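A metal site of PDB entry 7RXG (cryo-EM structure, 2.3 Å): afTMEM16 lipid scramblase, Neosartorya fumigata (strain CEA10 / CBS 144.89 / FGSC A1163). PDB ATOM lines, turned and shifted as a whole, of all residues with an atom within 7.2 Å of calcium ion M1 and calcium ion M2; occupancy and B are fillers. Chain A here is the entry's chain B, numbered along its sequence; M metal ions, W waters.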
ATOM      1  N   TYR A 180     -38.900 -30.173  -6.507  1.00  0.00           N
ATOM      2  CA  TYR A 180     -38.078 -29.846  -7.673  1.00  0.00           C
ATOM      3  C   TYR A 180     -37.548 -31.108  -8.344  1.00  0.00           C
ATOM      4  O   TYR A 180     -37.597 -31.228  -9.567  1.00  0.00           O
ATOM      5  CB  TYR A 180     -36.920 -28.933  -7.308  1.00  0.00           C
ATOM      6  CG  TYR A 180     -35.848 -28.941  -8.372  1.00  0.00           C
ATOM      7  CD1 TYR A 180     -36.091 -28.423  -9.635  1.00  0.00           C
ATOM      8  CD2 TYR A 180     -34.597 -29.505  -8.133  1.00  0.00           C
ATOM      9  CE1 TYR A 180     -35.134 -28.440 -10.621  1.00  0.00           C
ATOM     10  CE2 TYR A 180     -33.633 -29.522  -9.107  1.00  0.00           C
ATOM     11  CZ  TYR A 180     -33.902 -28.992 -10.347  1.00  0.00           C
ATOM     12  OH  TYR A 180     -32.938 -29.009 -11.321  1.00  0.00           O
ATOM     13  N   LEU A 184     -38.371 -32.485 -12.053  1.00  0.00           N
ATOM     14  CA  LEU A 184     -37.314 -32.727 -13.022  1.00  0.00           C
ATOM     15  C   LEU A 184     -37.370 -34.153 -13.554  1.00  0.00           C
ATOM     16  O   LEU A 184     -37.206 -34.373 -14.755  1.00  0.00           O
ATOM     17  CB  LEU A 184     -35.951 -32.432 -12.409  1.00  0.00           C
ATOM     18  CG  LEU A 184     -34.741 -32.536 -13.341  1.00  0.00           C
ATOM     19  CD1 LEU A 184     -34.963 -31.762 -14.611  1.00  0.00           C
ATOM     20  CD2 LEU A 184     -33.484 -32.079 -12.641  1.00  0.00           C
ATOM     21  N   ALA A 437     -25.570 -23.313 -24.843  1.00  0.00           N
ATOM     22  CA  ALA A 437     -25.944 -22.690 -23.588  1.00  0.00           C
ATOM     23  C   ALA A 437     -26.135 -23.734 -22.494  1.00  0.00           C
ATOM     24  O   ALA A 437     -25.772 -23.487 -21.346  1.00  0.00           O
ATOM     25  CB  ALA A 437     -27.199 -21.851 -23.754  1.00  0.00           C
ATOM     26  N   GLN A 438     -26.679 -24.908 -22.836  1.00  0.00           N
ATOM     27  CA  GLN A 438     -26.834 -25.959 -21.838  1.00  0.00           C
ATOM     28  C   GLN A 438     -25.479 -26.437 -21.316  1.00  0.00           C
ATOM     29  O   GLN A 438     -25.294 -26.571 -20.106  1.00  0.00           O
ATOM     30  CB  GLN A 438     -27.613 -27.140 -22.426  1.00  0.00           C
ATOM     31  CG  GLN A 438     -28.881 -26.776 -23.138  1.00  0.00           C
ATOM     32  CD  GLN A 438     -29.941 -26.232 -22.205  1.00  0.00           C
ATOM     33  OE1 GLN A 438     -30.336 -25.075 -22.305  1.00  0.00           O
ATOM     34  NE2 GLN A 438     -30.407 -27.073 -21.295  1.00  0.00           N
ATOM     35  N   ILE A 439     -24.526 -26.678 -22.223  1.00  0.00           N
ATOM     36  CA  ILE A 439     -23.213 -27.149 -21.792  1.00  0.00           C
ATOM     37  C   ILE A 439     -22.483 -26.070 -20.991  1.00  0.00           C
ATOM     38  O   ILE A 439     -21.897 -26.349 -19.937  1.00  0.00           O
ATOM     39  CB  ILE A 439     -22.395 -27.603 -23.019  1.00  0.00           C
ATOM     40  CG1 ILE A 439     -23.097 -28.758 -23.728  1.00  0.00           C
ATOM     41  CG2 ILE A 439     -20.995 -28.010 -22.592  1.00  0.00           C
ATOM     42  CD1 ILE A 439     -22.606 -29.008 -25.124  1.00  0.00           C
ATOM     43  N   VAL A 440     -22.507 -24.829 -21.473  1.00  0.00           N
ATOM     44  CA  VAL A 440     -21.820 -23.752 -20.778  1.00  0.00           C
ATOM     45  C   VAL A 440     -22.472 -23.473 -19.426  1.00  0.00           C
ATOM     46  O   VAL A 440     -21.793 -23.121 -18.461  1.00  0.00           O
ATOM     47  CB  VAL A 440     -21.786 -22.486 -21.658  1.00  0.00           C
ATOM     48  CG1 VAL A 440     -21.228 -21.317 -20.887  1.00  0.00           C
ATOM     49  CG2 VAL A 440     -20.967 -22.748 -22.912  1.00  0.00           C
ATOM     50  N   GLY A 441     -23.796 -23.633 -19.339  1.00  0.00           N
ATOM     51  CA  GLY A 441     -24.467 -23.445 -18.072  1.00  0.00           C
ATOM     52  C   GLY A 441     -24.177 -24.564 -17.093  1.00  0.00           C
ATOM     53  O   GLY A 441     -24.032 -24.303 -15.905  1.00  0.00           O
ATOM     54  N   PHE A 442     -24.076 -25.791 -17.582  1.00  0.00           N
ATOM     55  CA  PHE A 442     -23.604 -26.881 -16.728  1.00  0.00           C
ATOM     56  C   PHE A 442     -22.220 -26.567 -16.170  1.00  0.00           C
ATOM     57  O   PHE A 442     -21.980 -26.739 -14.967  1.00  0.00           O
ATOM     58  CB  PHE A 442     -23.569 -28.190 -17.515  1.00  0.00           C
ATOM     59  CG  PHE A 442     -22.759 -29.275 -16.872  1.00  0.00           C
ATOM     60  CD1 PHE A 442     -23.289 -30.028 -15.835  1.00  0.00           C
ATOM     61  CD2 PHE A 442     -21.473 -29.542 -17.302  1.00  0.00           C
ATOM     62  CE1 PHE A 442     -22.540 -31.023 -15.240  1.00  0.00           C
ATOM     63  CE2 PHE A 442     -20.726 -30.541 -16.698  1.00  0.00           C
ATOM     64  CZ  PHE A 442     -21.266 -31.282 -15.679  1.00  0.00           C
ATOM     65  N   ALA A 443     -21.324 -26.083 -17.027  1.00  0.00           N
ATOM     66  CA  ALA A 443     -19.989 -25.693 -16.564  1.00  0.00           C
ATOM     67  C   ALA A 443     -20.072 -24.619 -15.490  1.00  0.00           C
ATOM     68  O   ALA A 443     -19.651 -24.830 -14.354  1.00  0.00           O
ATOM     69  CB  ALA A 443     -19.138 -25.223 -17.741  1.00  0.00           C
ATOM     70  N   GLU A 445     -22.391 -23.702 -13.649  1.00  0.00           N
ATOM     71  CA  GLU A 445     -23.245 -24.038 -12.513  1.00  0.00           C
ATOM     72  C   GLU A 445     -22.583 -25.034 -11.569  1.00  0.00           C
ATOM     73  O   GLU A 445     -22.691 -24.872 -10.352  1.00  0.00           O
ATOM     74  CB  GLU A 445     -24.572 -24.592 -13.013  1.00  0.00           C
ATOM     75  CG  GLU A 445     -25.593 -24.850 -11.935  1.00  0.00           C
ATOM     76  CD  GLU A 445     -26.927 -25.287 -12.505  1.00  0.00           C
ATOM     77  OE1 GLU A 445     -27.005 -25.550 -13.717  1.00  0.00           O
ATOM     78  OE2 GLU A 445     -27.902 -25.364 -11.738  1.00  0.00           O
ATOM     79  N   THR A 446     -21.925 -26.065 -12.090  1.00  0.00           N
ATOM     80  CA  THR A 446     -21.307 -27.067 -11.243  1.00  0.00           C
ATOM     81  C   THR A 446     -19.791 -26.946 -11.165  1.00  0.00           C
ATOM     82  O   THR A 446     -19.241 -27.008 -10.067  1.00  0.00           O
ATOM     83  CB  THR A 446     -21.671 -28.478 -11.714  1.00  0.00           C
ATOM     84  OG1 THR A 446     -21.154 -28.690 -13.036  1.00  0.00           O
ATOM     85  CG2 THR A 446     -23.168 -28.674 -11.712  1.00  0.00           C
ATOM     86  N   TYR A 506     -28.201 -22.715  -1.105  1.00  0.00           N
ATOM     87  CA  TYR A 506     -28.970 -23.265  -2.211  1.00  0.00           C
ATOM     88  C   TYR A 506     -30.371 -22.675  -2.253  1.00  0.00           C
ATOM     89  O   TYR A 506     -31.065 -22.622  -1.235  1.00  0.00           O
ATOM     90  CB  TYR A 506     -29.051 -24.789  -2.108  1.00  0.00           C
ATOM     91  CG  TYR A 506     -29.855 -25.408  -3.217  1.00  0.00           C
ATOM     92  CD1 TYR A 506     -29.377 -25.432  -4.518  1.00  0.00           C
ATOM     93  CD2 TYR A 506     -31.109 -25.953  -2.977  1.00  0.00           C
ATOM     94  CE1 TYR A 506     -30.113 -25.992  -5.537  1.00  0.00           C
ATOM     95  CE2 TYR A 506     -31.854 -26.522  -3.990  1.00  0.00           C
ATOM     96  CZ  TYR A 506     -31.343 -26.533  -5.269  1.00  0.00           C
ATOM     97  OH  TYR A 506     -32.079 -27.093  -6.288  1.00  0.00           O
ATOM     98  N   ASP A 510     -33.791 -21.197  -8.328  1.00  0.00           N
ATOM     99  CA  ASP A 510     -32.892 -21.050  -9.471  1.00  0.00           C
ATOM    100  C   ASP A 510     -32.975 -22.246 -10.403  1.00  0.00           C
ATOM    101  O   ASP A 510     -33.036 -22.097 -11.622  1.00  0.00           O
ATOM    102  CB  ASP A 510     -31.460 -20.848  -8.998  1.00  0.00           C
ATOM    103  CG  ASP A 510     -31.326 -19.699  -8.014  1.00  0.00           C
ATOM    104  OD1 ASP A 510     -32.032 -18.689  -8.190  1.00  0.00           O
ATOM    105  OD2 ASP A 510     -30.523 -19.811  -7.075  1.00  0.00           O
ATOM    106  N   ASP A 511     -32.995 -23.457  -9.838  1.00  0.00           N
ATOM    107  CA  ASP A 511     -33.072 -24.651 -10.658  1.00  0.00           C
ATOM    108  C   ASP A 511     -34.429 -24.764 -11.335  1.00  0.00           C
ATOM    109  O   ASP A 511     -34.527 -25.160 -12.507  1.00  0.00           O
ATOM    110  CB  ASP A 511     -32.771 -25.887  -9.815  1.00  0.00           C
ATOM    111  CG  ASP A 511     -31.297 -26.011  -9.486  1.00  0.00           C
ATOM    112  OD1 ASP A 511     -30.484 -25.381 -10.172  1.00  0.00           O
ATOM    113  OD2 ASP A 511     -30.954 -26.747  -8.543  1.00  0.00           O
ATOM    114  N   LEU A 512     -35.494 -24.415 -10.618  1.00  0.00           N
ATOM    115  CA  LEU A 512     -36.819 -24.396 -11.233  1.00  0.00           C
ATOM    116  C   LEU A 512     -36.889 -23.384 -12.369  1.00  0.00           C
ATOM    117  O   LEU A 512     -37.469 -23.660 -13.418  1.00  0.00           O
ATOM    118  CB  LEU A 512     -37.896 -24.120 -10.187  1.00  0.00           C
ATOM    119  CG  LEU A 512     -38.253 -25.301  -9.296  1.00  0.00           C
ATOM    120  CD1 LEU A 512     -38.933 -24.807  -8.021  1.00  0.00           C
ATOM    121  CD2 LEU A 512     -39.131 -26.284 -10.034  1.00  0.00           C
ATOM    122  N   GLU A 514     -34.375 -22.384 -14.237  1.00  0.00           N
ATOM    123  CA  GLU A 514     -33.621 -22.921 -15.366  1.00  0.00           C
ATOM    124  C   GLU A 514     -34.445 -23.946 -16.136  1.00  0.00           C
ATOM    125  O   GLU A 514     -34.514 -23.890 -17.374  1.00  0.00           O
ATOM    126  CB  GLU A 514     -32.317 -23.538 -14.879  1.00  0.00           C
ATOM    127  CG  GLU A 514     -31.492 -24.153 -15.976  1.00  0.00           C
ATOM    128  CD  GLU A 514     -30.322 -24.965 -15.470  1.00  0.00           C
ATOM    129  OE1 GLU A 514     -29.945 -24.791 -14.297  1.00  0.00           O
ATOM    130  OE2 GLU A 514     -29.783 -25.772 -16.253  1.00  0.00           O
ATOM    131  N   MET A 515     -35.090 -24.871 -15.431  1.00  0.00           N
ATOM    132  CA  MET A 515     -35.889 -25.882 -16.125  1.00  0.00           C
ATOM    133  C   MET A 515     -37.083 -25.278 -16.844  1.00  0.00           C
ATOM    134  O   MET A 515     -37.432 -25.716 -17.940  1.00  0.00           O
ATOM    135  CB  MET A 515     -36.336 -26.967 -15.141  1.00  0.00           C
ATOM    136  CG  MET A 515     -35.214 -27.916 -14.745  1.00  0.00           C
ATOM    137  SD  MET A 515     -34.420 -28.720 -16.159  1.00  0.00           S
ATOM    138  CE  MET A 515     -32.949 -27.729 -16.330  1.00  0.00           C
ATOM    139  N   GLN A 518     -35.878 -23.569 -20.007  1.00  0.00           N
ATOM    140  CA  GLN A 518     -35.600 -24.606 -20.992  1.00  0.00           C
ATOM    141  C   GLN A 518     -36.885 -25.107 -21.649  1.00  0.00           C
ATOM    142  O   GLN A 518     -36.960 -25.264 -22.880  1.00  0.00           O
ATOM    143  CB  GLN A 518     -34.844 -25.743 -20.325  1.00  0.00           C
ATOM    144  CG  GLN A 518     -34.342 -26.797 -21.263  1.00  0.00           C
ATOM    145  CD  GLN A 518     -34.127 -28.126 -20.582  1.00  0.00           C
ATOM    146  OE1 GLN A 518     -35.065 -28.874 -20.372  1.00  0.00           O
ATOM    147  NE2 GLN A 518     -32.888 -28.410 -20.225  1.00  0.00           N
ATOM    148  N   ASN A 539     -29.591 -33.431 -21.408  1.00  0.00           N
ATOM    149  CA  ASN A 539     -29.206 -32.452 -20.415  1.00  0.00           C
ATOM    150  C   ASN A 539     -29.949 -32.663 -19.100  1.00  0.00           C
ATOM    151  O   ASN A 539     -29.389 -32.427 -18.038  1.00  0.00           O
ATOM    152  CB  ASN A 539     -29.455 -31.034 -20.920  1.00  0.00           C
ATOM    153  CG  ASN A 539     -29.174 -29.980 -19.867  1.00  0.00           C
ATOM    154  OD1 ASN A 539     -28.042 -29.544 -19.711  1.00  0.00           O
ATOM    155  ND2 ASN A 539     -30.201 -29.578 -19.132  1.00  0.00           N
ATOM    156  N   GLU A 543     -28.856 -33.311 -15.517  1.00  0.00           N
ATOM    157  CA  GLU A 543     -29.219 -32.218 -14.629  1.00  0.00           C
ATOM    158  C   GLU A 543     -29.654 -32.721 -13.273  1.00  0.00           C
ATOM    159  O   GLU A 543     -29.325 -32.112 -12.250  1.00  0.00           O
ATOM    160  CB  GLU A 543     -30.335 -31.380 -15.258  1.00  0.00           C
ATOM    161  CG  GLU A 543     -30.604 -30.067 -14.570  1.00  0.00           C
ATOM    162  CD  GLU A 543     -29.623 -28.996 -14.976  1.00  0.00           C
ATOM    163  OE1 GLU A 543     -29.311 -28.117 -14.136  1.00  0.00           O
ATOM    164  OE2 GLU A 543     -29.153 -29.016 -16.124  1.00  0.00           O
ATOM    165  N   SER A 546     -26.328 -33.731 -11.535  1.00  0.00           N
ATOM    166  CA  SER A 546     -25.448 -32.597 -11.271  1.00  0.00           C
ATOM    167  C   SER A 546     -26.051 -31.607 -10.288  1.00  0.00           C
ATOM    168  O   SER A 546     -25.322 -31.006  -9.505  1.00  0.00           O
ATOM    169  CB  SER A 546     -25.076 -31.914 -12.592  1.00  0.00           C
ATOM    170  OG  SER A 546     -26.048 -30.958 -12.962  1.00  0.00           O
ATOM    171  N   ASP A 547     -27.375 -31.458 -10.287  1.00  0.00           N
ATOM    172  CA  ASP A 547     -28.013 -30.602  -9.289  1.00  0.00           C
ATOM    173  C   ASP A 547     -27.946 -31.230  -7.902  1.00  0.00           C
ATOM    174  O   ASP A 547     -27.730 -30.531  -6.912  1.00  0.00           O
ATOM    175  CB  ASP A 547     -29.455 -30.304  -9.682  1.00  0.00           C
ATOM    176  CG  ASP A 547     -29.571 -29.149 -10.642  1.00  0.00           C
ATOM    177  OD1 ASP A 547     -28.601 -28.387 -10.765  1.00  0.00           O
ATOM    178  OD2 ASP A 547     -30.630 -29.014 -11.279  1.00  0.00           O
ATOM    179  N   LYS A 550     -24.470 -30.611  -6.772  1.00  0.00           N
ATOM    180  CA  LYS A 550     -24.304 -29.220  -6.371  1.00  0.00           C
ATOM    181  C   LYS A 550     -24.892 -28.974  -4.991  1.00  0.00           C
ATOM    182  O   LYS A 550     -24.307 -28.265  -4.172  1.00  0.00           O
ATOM    183  CB  LYS A 550     -24.959 -28.299  -7.402  1.00  0.00           C
ATOM    184  CG  LYS A 550     -24.996 -26.846  -7.004  1.00  0.00           C
ATOM    185  CD  LYS A 550     -25.680 -26.024  -8.081  1.00  0.00           C
ATOM    186  CE  LYS A 550     -27.158 -26.328  -8.155  1.00  0.00           C
ATOM    187  NZ  LYS A 550     -27.848 -25.496  -9.162  1.00  0.00           N
HETATM  188 CA    CA M   1     -29.860 -26.602 -12.360  1.00  0.00          CA
HETATM  189 CA    CA M   2     -27.665 -26.826 -15.843  1.00  0.00          CA
HETATM  190  O   HOH W   1     -27.433 -27.509 -18.265  1.00  0.00           O
HETATM  191  O   HOH W   2     -32.290 -27.008 -13.255  1.00  0.00           O
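Water W2 lies within hydrogen-bond range of OH of Tyr 180 (2.9 Å) and O of Asp 511 (3.0 Å). Water W1 bridges the side-chain amide oxygen (OD1) of Asn 539 and the backbone carbonyl oxygen (O) of Gln 438.
Calcium ion M2 is bound by OE2 of Glu 514 (2.4 Å), water W1 (2.5 Å), OE1 of Glu 445 (2.6 Å), OE2 of Glu 543 (2.7 Å) and OE1 of Glu 543 (2.7 Å). Calcium ion M2 has five donor atoms within binding distance.
The side-chain hydroxyl (OH) of Tyr 506 is in hydrogen-bond range of the side-chain carboxylate (OD2) of Asp 511, 2.5 Å away. OD2 of Asp 511 is in salt-bridge range of NZ of Lys 550, 3.4 Å away. OE2 of Glu 445 lies close to NZ of Lys 550 (2.6 Å). The side-chain carboxylate of Glu 543 sits close to the side-chain amide nitrogen of Asn 539 (3.2 Å). The side-chain carboxylate (OD1) of Asp 547 sits close to the side-chain amino group (NZ) of Lys 550, 3.4 Å away.
Lys 550 touches calcium ion M1 (NZ to CA, 3.9 Å). Six residues have an atom within 4 Å of calcium ion M1: Glu 445, Asp 511, Glu 514, Glu 543, Asp 547 and Lys 550.
Calcium ion M1 is bound by OE1 of Glu 543, OE2 of Glu 445, OD1 of Asp 511, water W2, OE1 of Glu 514, OD1 of Asp 547 and OD2 of Asp 547.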
